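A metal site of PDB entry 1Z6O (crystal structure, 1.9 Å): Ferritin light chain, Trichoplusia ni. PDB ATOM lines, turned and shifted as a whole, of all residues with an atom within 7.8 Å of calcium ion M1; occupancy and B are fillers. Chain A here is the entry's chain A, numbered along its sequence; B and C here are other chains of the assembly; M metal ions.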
ATOM      1  N   HIS A 144       7.342 -14.850 -10.442  1.00  0.00           N
ATOM      2  CA  HIS A 144       6.361 -15.157  -9.414  1.00  0.00           C
ATOM      3  C   HIS A 144       5.953 -13.857  -8.688  1.00  0.00           C
ATOM      4  O   HIS A 144       4.774 -13.602  -8.448  1.00  0.00           O
ATOM      5  CB  HIS A 144       6.975 -16.164  -8.430  1.00  0.00           C
ATOM      6  CG  HIS A 144       6.027 -16.683  -7.399  1.00  0.00           C
ATOM      7  ND1 HIS A 144       5.625 -15.943  -6.303  1.00  0.00           N
ATOM      8  CD2 HIS A 144       5.415 -17.886  -7.280  1.00  0.00           C
ATOM      9  CE1 HIS A 144       4.819 -16.667  -5.553  1.00  0.00           C
ATOM     10  NE2 HIS A 144       4.674 -17.857  -6.120  1.00  0.00           N
ATOM     11  N   PRO A 157      -2.497 -16.033  -9.893  1.00  0.00           N
ATOM     12  CA  PRO A 157      -2.038 -17.189  -9.129  1.00  0.00           C
ATOM     13  C   PRO A 157      -1.886 -18.458  -9.973  1.00  0.00           C
ATOM     14  O   PRO A 157      -1.315 -19.439  -9.501  1.00  0.00           O
ATOM     15  CB  PRO A 157      -3.089 -17.323  -8.022  1.00  0.00           C
ATOM     16  CG  PRO A 157      -4.337 -16.785  -8.660  1.00  0.00           C
ATOM     17  CD  PRO A 157      -3.851 -15.599  -9.478  1.00  0.00           C
ATOM     18  N   ALA A 160       1.646 -18.244 -10.819  1.00  0.00           N
ATOM     19  CA  ALA A 160       2.382 -18.493  -9.573  1.00  0.00           C
ATOM     20  C   ALA A 160       2.435 -19.982  -9.220  1.00  0.00           C
ATOM     21  O   ALA A 160       3.502 -20.519  -8.915  1.00  0.00           O
ATOM     22  CB  ALA A 160       1.762 -17.695  -8.413  1.00  0.00           C
ATOM     23  N   GLN A 161       1.287 -20.667  -9.275  1.00  0.00           N
ATOM     24  CA  GLN A 161       1.231 -22.087  -8.935  1.00  0.00           C
ATOM     25  C   GLN A 161       2.000 -22.916  -9.986  1.00  0.00           C
ATOM     26  O   GLN A 161       2.650 -23.900  -9.628  1.00  0.00           O
ATOM     27  CB  GLN A 161      -0.231 -22.565  -8.842  1.00  0.00           C
ATOM     28  CG  GLN A 161      -0.396 -24.090  -8.794  1.00  0.00           C
ATOM     29  CD  GLN A 161      -0.114 -24.735  -7.421  1.00  0.00           C
ATOM     30  OE1 GLN A 161       0.550 -24.159  -6.538  1.00  0.00           O
ATOM     31  NE2 GLN A 161      -0.594 -25.958  -7.253  1.00  0.00           N
ATOM     32  N   TYR A 162       1.913 -22.519 -11.246  1.00  0.00           N
ATOM     33  CA  TYR A 162       2.663 -23.216 -12.309  1.00  0.00           C
ATOM     34  C   TYR A 162       4.170 -23.143 -12.003  1.00  0.00           C
ATOM     35  O   TYR A 162       4.878 -24.156 -12.056  1.00  0.00           O
ATOM     36  CB  TYR A 162       2.368 -22.558 -13.668  1.00  0.00           C
ATOM     37  CG  TYR A 162       3.264 -23.030 -14.801  1.00  0.00           C
ATOM     38  CD1 TYR A 162       3.312 -24.375 -15.181  1.00  0.00           C
ATOM     39  CD2 TYR A 162       4.032 -22.112 -15.519  1.00  0.00           C
ATOM     40  CE1 TYR A 162       4.116 -24.790 -16.266  1.00  0.00           C
ATOM     41  CE2 TYR A 162       4.832 -22.515 -16.596  1.00  0.00           C
ATOM     42  CZ  TYR A 162       4.860 -23.847 -16.956  1.00  0.00           C
ATOM     43  OH  TYR A 162       5.651 -24.229 -18.017  1.00  0.00           O
ATOM     44  N   GLU A 164       5.583 -22.530  -9.060  1.00  0.00           N
ATOM     45  CA  GLU A 164       5.830 -23.250  -7.817  1.00  0.00           C
ATOM     46  C   GLU A 164       5.966 -24.748  -8.034  1.00  0.00           C
ATOM     47  O   GLU A 164       6.896 -25.377  -7.548  1.00  0.00           O
ATOM     48  CB  GLU A 164       4.688 -22.994  -6.805  1.00  0.00           C
ATOM     49  CG  GLU A 164       4.724 -21.565  -6.230  1.00  0.00           C
ATOM     50  CD  GLU A 164       3.465 -21.195  -5.446  1.00  0.00           C
ATOM     51  OE1 GLU A 164       2.605 -22.059  -5.194  1.00  0.00           O
ATOM     52  OE2 GLU A 164       3.333 -19.999  -5.087  1.00  0.00           O
ATOM     53  N   GLU A 165       5.026 -25.305  -8.785  1.00  0.00           N
ATOM     54  CA  GLU A 165       4.994 -26.738  -9.044  1.00  0.00           C
ATOM     55  C   GLU A 165       6.019 -27.281 -10.049  1.00  0.00           C
ATOM     56  O   GLU A 165       6.644 -28.312  -9.815  1.00  0.00           O
ATOM     57  CB  GLU A 165       3.598 -27.134  -9.554  1.00  0.00           C
ATOM     58  CG  GLU A 165       2.470 -26.958  -8.552  1.00  0.00           C
ATOM     59  CD  GLU A 165       2.427 -28.098  -7.554  1.00  0.00           C
ATOM     60  OE1 GLU A 165       2.888 -29.200  -7.919  1.00  0.00           O
ATOM     61  OE2 GLU A 165       1.926 -27.901  -6.423  1.00  0.00           O
ATOM     62  N   GLU A 169      10.145 -25.851  -6.854  1.00  0.00           N
ATOM     63  CA  GLU A 169      10.471 -26.958  -5.944  1.00  0.00           C
ATOM     64  C   GLU A 169      11.758 -27.654  -6.358  1.00  0.00           C
ATOM     65  O   GLU A 169      12.641 -27.868  -5.520  1.00  0.00           O
ATOM     66  CB  GLU A 169       9.364 -28.008  -5.925  1.00  0.00           C
ATOM     67  CG  GLU A 169       7.980 -27.488  -5.628  1.00  0.00           C
ATOM     68  CD  GLU A 169       6.949 -28.615  -5.554  1.00  0.00           C
ATOM     69  OE1 GLU A 169       6.970 -29.501  -6.445  1.00  0.00           O
ATOM     70  OE2 GLU A 169       6.113 -28.601  -4.623  1.00  0.00           O
ATOM     71  N   HIS B 144       5.057 -17.972   6.175  1.00  0.00           N
ATOM     72  CA  HIS B 144       4.615 -17.813   4.789  1.00  0.00           C
ATOM     73  C   HIS B 144       4.477 -16.311   4.470  1.00  0.00           C
ATOM     74  O   HIS B 144       4.918 -15.841   3.414  1.00  0.00           O
ATOM     75  CB  HIS B 144       3.282 -18.538   4.612  1.00  0.00           C
ATOM     76  CG  HIS B 144       2.780 -18.581   3.201  1.00  0.00           C
ATOM     77  ND1 HIS B 144       2.216 -17.495   2.571  1.00  0.00           N
ATOM     78  CD2 HIS B 144       2.734 -19.605   2.309  1.00  0.00           C
ATOM     79  CE1 HIS B 144       1.841 -17.845   1.350  1.00  0.00           C
ATOM     80  NE2 HIS B 144       2.146 -19.120   1.164  1.00  0.00           N
ATOM     81  N   PRO B 157       9.271 -17.622  -2.805  1.00  0.00           N
ATOM     82  CA  PRO B 157       8.170 -18.540  -3.057  1.00  0.00           C
ATOM     83  C   PRO B 157       8.542 -20.006  -2.893  1.00  0.00           C
ATOM     84  O   PRO B 157       7.663 -20.870  -2.873  1.00  0.00           O
ATOM     85  CB  PRO B 157       7.726 -18.183  -4.484  1.00  0.00           C
ATOM     86  CG  PRO B 157       9.002 -17.702  -5.125  1.00  0.00           C
ATOM     87  CD  PRO B 157       9.690 -16.902  -4.031  1.00  0.00           C
ATOM     88  N   ALA B 160       7.524 -20.527   0.566  1.00  0.00           N
ATOM     89  CA  ALA B 160       6.060 -20.477   0.576  1.00  0.00           C
ATOM     90  C   ALA B 160       5.428 -21.788   0.064  1.00  0.00           C
ATOM     91  O   ALA B 160       4.527 -22.337   0.703  1.00  0.00           O
ATOM     92  CB  ALA B 160       5.561 -19.297  -0.265  1.00  0.00           C
ATOM     93  N   GLN B 161       5.916 -22.287  -1.069  1.00  0.00           N
ATOM     94  CA  GLN B 161       5.364 -23.525  -1.647  1.00  0.00           C
ATOM     95  C   GLN B 161       5.687 -24.716  -0.751  1.00  0.00           C
ATOM     96  O   GLN B 161       4.866 -25.635  -0.603  1.00  0.00           O
ATOM     97  CB  GLN B 161       5.927 -23.751  -3.063  1.00  0.00           C
ATOM     98  CG  GLN B 161       5.647 -25.151  -3.636  1.00  0.00           C
ATOM     99  CD  GLN B 161       4.219 -25.374  -4.169  1.00  0.00           C
ATOM    100  OE1 GLN B 161       3.263 -24.642  -3.844  1.00  0.00           O
ATOM    101  NE2 GLN B 161       4.071 -26.410  -4.990  1.00  0.00           N
ATOM    102  N   TYR B 162       6.872 -24.726  -0.142  1.00  0.00           N
ATOM    103  CA  TYR B 162       7.254 -25.811   0.769  1.00  0.00           C
ATOM    104  C   TYR B 162       6.249 -25.849   1.947  1.00  0.00           C
ATOM    105  O   TYR B 162       5.744 -26.913   2.311  1.00  0.00           O
ATOM    106  CB  TYR B 162       8.672 -25.574   1.303  1.00  0.00           C
ATOM    107  CG  TYR B 162       9.088 -26.478   2.450  1.00  0.00           C
ATOM    108  CD1 TYR B 162       9.110 -27.873   2.305  1.00  0.00           C
ATOM    109  CD2 TYR B 162       9.485 -25.949   3.669  1.00  0.00           C
ATOM    110  CE1 TYR B 162       9.522 -28.708   3.360  1.00  0.00           C
ATOM    111  CE2 TYR B 162       9.908 -26.764   4.715  1.00  0.00           C
ATOM    112  CZ  TYR B 162       9.927 -28.133   4.559  1.00  0.00           C
ATOM    113  OH  TYR B 162      10.343 -28.925   5.608  1.00  0.00           O
ATOM    114  N   GLU B 164       3.197 -24.553   2.013  1.00  0.00           N
ATOM    115  CA  GLU B 164       1.875 -24.873   1.480  1.00  0.00           C
ATOM    116  C   GLU B 164       1.685 -26.374   1.300  1.00  0.00           C
ATOM    117  O   GLU B 164       0.681 -26.937   1.716  1.00  0.00           O
ATOM    118  CB  GLU B 164       1.655 -24.168   0.124  1.00  0.00           C
ATOM    119  CG  GLU B 164       1.443 -22.655   0.268  1.00  0.00           C
ATOM    120  CD  GLU B 164       1.499 -21.891  -1.054  1.00  0.00           C
ATOM    121  OE1 GLU B 164       1.533 -22.524  -2.135  1.00  0.00           O
ATOM    122  OE2 GLU B 164       1.499 -20.644  -1.010  1.00  0.00           O
ATOM    123  N   GLU B 165       2.680 -27.013   0.676  1.00  0.00           N
ATOM    124  CA  GLU B 165       2.613 -28.434   0.382  1.00  0.00           C
ATOM    125  C   GLU B 165       2.833 -29.382   1.566  1.00  0.00           C
ATOM    126  O   GLU B 165       2.115 -30.365   1.720  1.00  0.00           O
ATOM    127  CB  GLU B 165       3.663 -28.774  -0.680  1.00  0.00           C
ATOM    128  CG  GLU B 165       3.416 -28.155  -2.049  1.00  0.00           C
ATOM    129  CD  GLU B 165       2.363 -28.914  -2.829  1.00  0.00           C
ATOM    130  OE1 GLU B 165       2.215 -30.124  -2.571  1.00  0.00           O
ATOM    131  OE2 GLU B 165       1.705 -28.315  -3.707  1.00  0.00           O
ATOM    132  N   GLU B 169      -1.624 -27.599   4.055  1.00  0.00           N
ATOM    133  CA  GLU B 169      -2.774 -28.400   3.635  1.00  0.00           C
ATOM    134  C   GLU B 169      -3.225 -29.350   4.728  1.00  0.00           C
ATOM    135  O   GLU B 169      -4.408 -29.415   5.068  1.00  0.00           O
ATOM    136  CB  GLU B 169      -2.455 -29.238   2.401  1.00  0.00           C
ATOM    137  CG  GLU B 169      -1.909 -28.479   1.218  1.00  0.00           C
ATOM    138  CD  GLU B 169      -1.682 -29.377   0.012  1.00  0.00           C
ATOM    139  OE1 GLU B 169      -1.129 -30.487   0.187  1.00  0.00           O
ATOM    140  OE2 GLU B 169      -2.045 -28.974  -1.111  1.00  0.00           O
ATOM    141  N   HIS C 144      -8.554 -15.607  -4.060  1.00  0.00           N
ATOM    142  CA  HIS C 144      -7.144 -15.822  -3.772  1.00  0.00           C
ATOM    143  C   HIS C 144      -6.487 -14.486  -3.352  1.00  0.00           C
ATOM    144  O   HIS C 144      -5.729 -14.420  -2.386  1.00  0.00           O
ATOM    145  CB  HIS C 144      -6.469 -16.398  -5.022  1.00  0.00           C
ATOM    146  CG  HIS C 144      -5.042 -16.806  -4.829  1.00  0.00           C
ATOM    147  ND1 HIS C 144      -4.001 -15.895  -4.760  1.00  0.00           N
ATOM    148  CD2 HIS C 144      -4.475 -18.042  -4.737  1.00  0.00           C
ATOM    149  CE1 HIS C 144      -2.858 -16.551  -4.627  1.00  0.00           C
ATOM    150  NE2 HIS C 144      -3.124 -17.853  -4.608  1.00  0.00           N
ATOM    151  N   PRO C 157      -3.044 -18.552   3.662  1.00  0.00           N
ATOM    152  CA  PRO C 157      -2.463 -19.357   2.587  1.00  0.00           C
ATOM    153  C   PRO C 157      -3.086 -20.732   2.448  1.00  0.00           C
ATOM    154  O   PRO C 157      -2.840 -21.431   1.470  1.00  0.00           O
ATOM    155  CB  PRO C 157      -0.967 -19.402   2.944  1.00  0.00           C
ATOM    156  CG  PRO C 157      -0.969 -19.306   4.443  1.00  0.00           C
ATOM    157  CD  PRO C 157      -2.070 -18.303   4.751  1.00  0.00           C
ATOM    158  N   ALA C 160      -5.596 -20.047  -0.094  1.00  0.00           N
ATOM    159  CA  ALA C 160      -4.866 -19.807  -1.344  1.00  0.00           C
ATOM    160  C   ALA C 160      -4.391 -21.119  -1.990  1.00  0.00           C
ATOM    161  O   ALA C 160      -4.586 -21.334  -3.192  1.00  0.00           O
ATOM    162  CB  ALA C 160      -3.663 -18.885  -1.090  1.00  0.00           C
ATOM    163  N   GLN C 161      -3.770 -22.001  -1.204  1.00  0.00           N
ATOM    164  CA  GLN C 161      -3.270 -23.273  -1.743  1.00  0.00           C
ATOM    165  C   GLN C 161      -4.434 -24.166  -2.173  1.00  0.00           C
ATOM    166  O   GLN C 161      -4.332 -24.880  -3.171  1.00  0.00           O
ATOM    167  CB  GLN C 161      -2.404 -23.990  -0.683  1.00  0.00           C
ATOM    168  CG  GLN C 161      -2.069 -25.455  -1.034  1.00  0.00           C
ATOM    169  CD  GLN C 161      -0.959 -25.647  -2.072  1.00  0.00           C
ATOM    170  OE1 GLN C 161      -0.600 -24.742  -2.848  1.00  0.00           O
ATOM    171  NE2 GLN C 161      -0.399 -26.851  -2.102  1.00  0.00           N
ATOM    172  N   TYR C 162      -5.536 -24.147  -1.419  1.00  0.00           N
ATOM    173  CA  TYR C 162      -6.726 -24.934  -1.793  1.00  0.00           C
ATOM    174  C   TYR C 162      -7.220 -24.479  -3.179  1.00  0.00           C
ATOM    175  O   TYR C 162      -7.481 -25.312  -4.059  1.00  0.00           O
ATOM    176  CB  TYR C 162      -7.828 -24.723  -0.750  1.00  0.00           C
ATOM    177  CG  TYR C 162      -9.184 -25.286  -1.140  1.00  0.00           C
ATOM    178  CD1 TYR C 162      -9.355 -26.637  -1.424  1.00  0.00           C
ATOM    179  CD2 TYR C 162     -10.300 -24.449  -1.200  1.00  0.00           C
ATOM    180  CE1 TYR C 162     -10.627 -27.162  -1.744  1.00  0.00           C
ATOM    181  CE2 TYR C 162     -11.565 -24.956  -1.516  1.00  0.00           C
ATOM    182  CZ  TYR C 162     -11.714 -26.307  -1.788  1.00  0.00           C
ATOM    183  OH  TYR C 162     -12.973 -26.783  -2.105  1.00  0.00           O
ATOM    184  N   GLU C 164      -5.476 -22.854  -5.493  1.00  0.00           N
ATOM    185  CA  GLU C 164      -4.432 -23.158  -6.469  1.00  0.00           C
ATOM    186  C   GLU C 164      -4.492 -24.605  -6.934  1.00  0.00           C
ATOM    187  O   GLU C 164      -4.457 -24.879  -8.131  1.00  0.00           O
ATOM    188  CB  GLU C 164      -3.037 -22.882  -5.876  1.00  0.00           C
ATOM    189  CG  GLU C 164      -2.742 -21.381  -5.723  1.00  0.00           C
ATOM    190  CD  GLU C 164      -1.504 -21.060  -4.893  1.00  0.00           C
ATOM    191  OE1 GLU C 164      -0.736 -21.989  -4.544  1.00  0.00           O
ATOM    192  OE2 GLU C 164      -1.285 -19.878  -4.583  1.00  0.00           O
ATOM    193  N   GLU C 165      -4.601 -25.512  -5.971  1.00  0.00           N
ATOM    194  CA  GLU C 165      -4.610 -26.944  -6.269  1.00  0.00           C
ATOM    195  C   GLU C 165      -5.909 -27.501  -6.857  1.00  0.00           C
ATOM    196  O   GLU C 165      -5.890 -28.298  -7.792  1.00  0.00           O
ATOM    197  CB  GLU C 165      -4.311 -27.726  -4.988  1.00  0.00           C
ATOM    198  CG  GLU C 165      -2.917 -27.519  -4.428  1.00  0.00           C
ATOM    199  CD  GLU C 165      -1.882 -28.342  -5.169  1.00  0.00           C
ATOM    200  OE1 GLU C 165      -2.271 -29.394  -5.731  1.00  0.00           O
ATOM    201  OE2 GLU C 165      -0.691 -27.963  -5.192  1.00  0.00           O
ATOM    202  N   GLU C 169      -5.405 -24.496 -11.320  1.00  0.00           N
ATOM    203  CA  GLU C 169      -4.652 -25.240 -12.331  1.00  0.00           C
ATOM    204  C   GLU C 169      -5.538 -25.748 -13.450  1.00  0.00           C
ATOM    205  O   GLU C 169      -5.243 -25.554 -14.629  1.00  0.00           O
ATOM    206  CB  GLU C 169      -3.941 -26.443 -11.724  1.00  0.00           C
ATOM    207  CG  GLU C 169      -3.062 -26.161 -10.534  1.00  0.00           C
ATOM    208  CD  GLU C 169      -2.345 -27.407 -10.029  1.00  0.00           C
ATOM    209  OE1 GLU C 169      -2.997 -28.471  -9.918  1.00  0.00           O
ATOM    210  OE2 GLU C 169      -1.134 -27.325  -9.736  1.00  0.00           O
HETATM  211 CA    CA M   1       1.200 -23.507  -4.185  1.00  0.00          CA
HETATM  212 CA    CA M   2       1.301 -18.106  -3.108  1.00  0.00          CA
HETATM  213 FE    FE M   3       1.043 -29.606  -5.383  1.00  0.00          FE
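OE2 of Glu 165 of chain C sits close to NE2 of Gln 161 of chain A (2.9 Å). The side-chain carboxylate (OE2) of Glu 164 of chain B lies within hydrogen-bond range of a ring nitrogen (NE2) of His 144 of chain B, 2.7 Å away. N of Glu 169 of chain C sits close to O of Glu 164 of chain C (3.3 Å). The side-chain carboxylate (OE2) of Glu 165 of chain A sits close to the side-chain amide nitrogen (NE2) of Gln 161 of chain B (3.0 Å). The side-chain carboxylate (OE2) of Glu 165 of chain A lies close to the side-chain amide nitrogen (NE2) of Gln 161 of chain A. OE2 of Glu 164 of chain C is in hydrogen-bond range of NE2 of His 144 of chain C (2.7 Å). The side-chain carboxylate (OE2) of Glu 169 of chain A is in hydrogen-bond range of the side-chain amide nitrogen (NE2) of Gln 161 of chain B (3.0 Å). The side-chain carboxylate (OE2) of Glu 165 of chain B lies close to the side-chain amide nitrogen (NE2) of Gln 161 of chain B (3.3 Å).
Of the 24 residues printed, 6 come within 4 Å of calcium ion M1.
Calcium ion M1 is bound by the side-chain carboxylate of Glu 164 of chain A (2.3 Å), the side-chain carboxylate of Glu 164 of chain B (2.3 Å), the side-chain amide oxygen of Gln 161 of chain B (2.4 Å), the side-chain carboxylate of Glu 164 of chain C (2.5 Å), the side-chain amide oxygen of Gln 161 of chain A (2.5 Å) and the side-chain amide oxygen of Gln 161 of chain C (2.6 Å). Calcium ion M1 has six donor atoms within binding distance.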
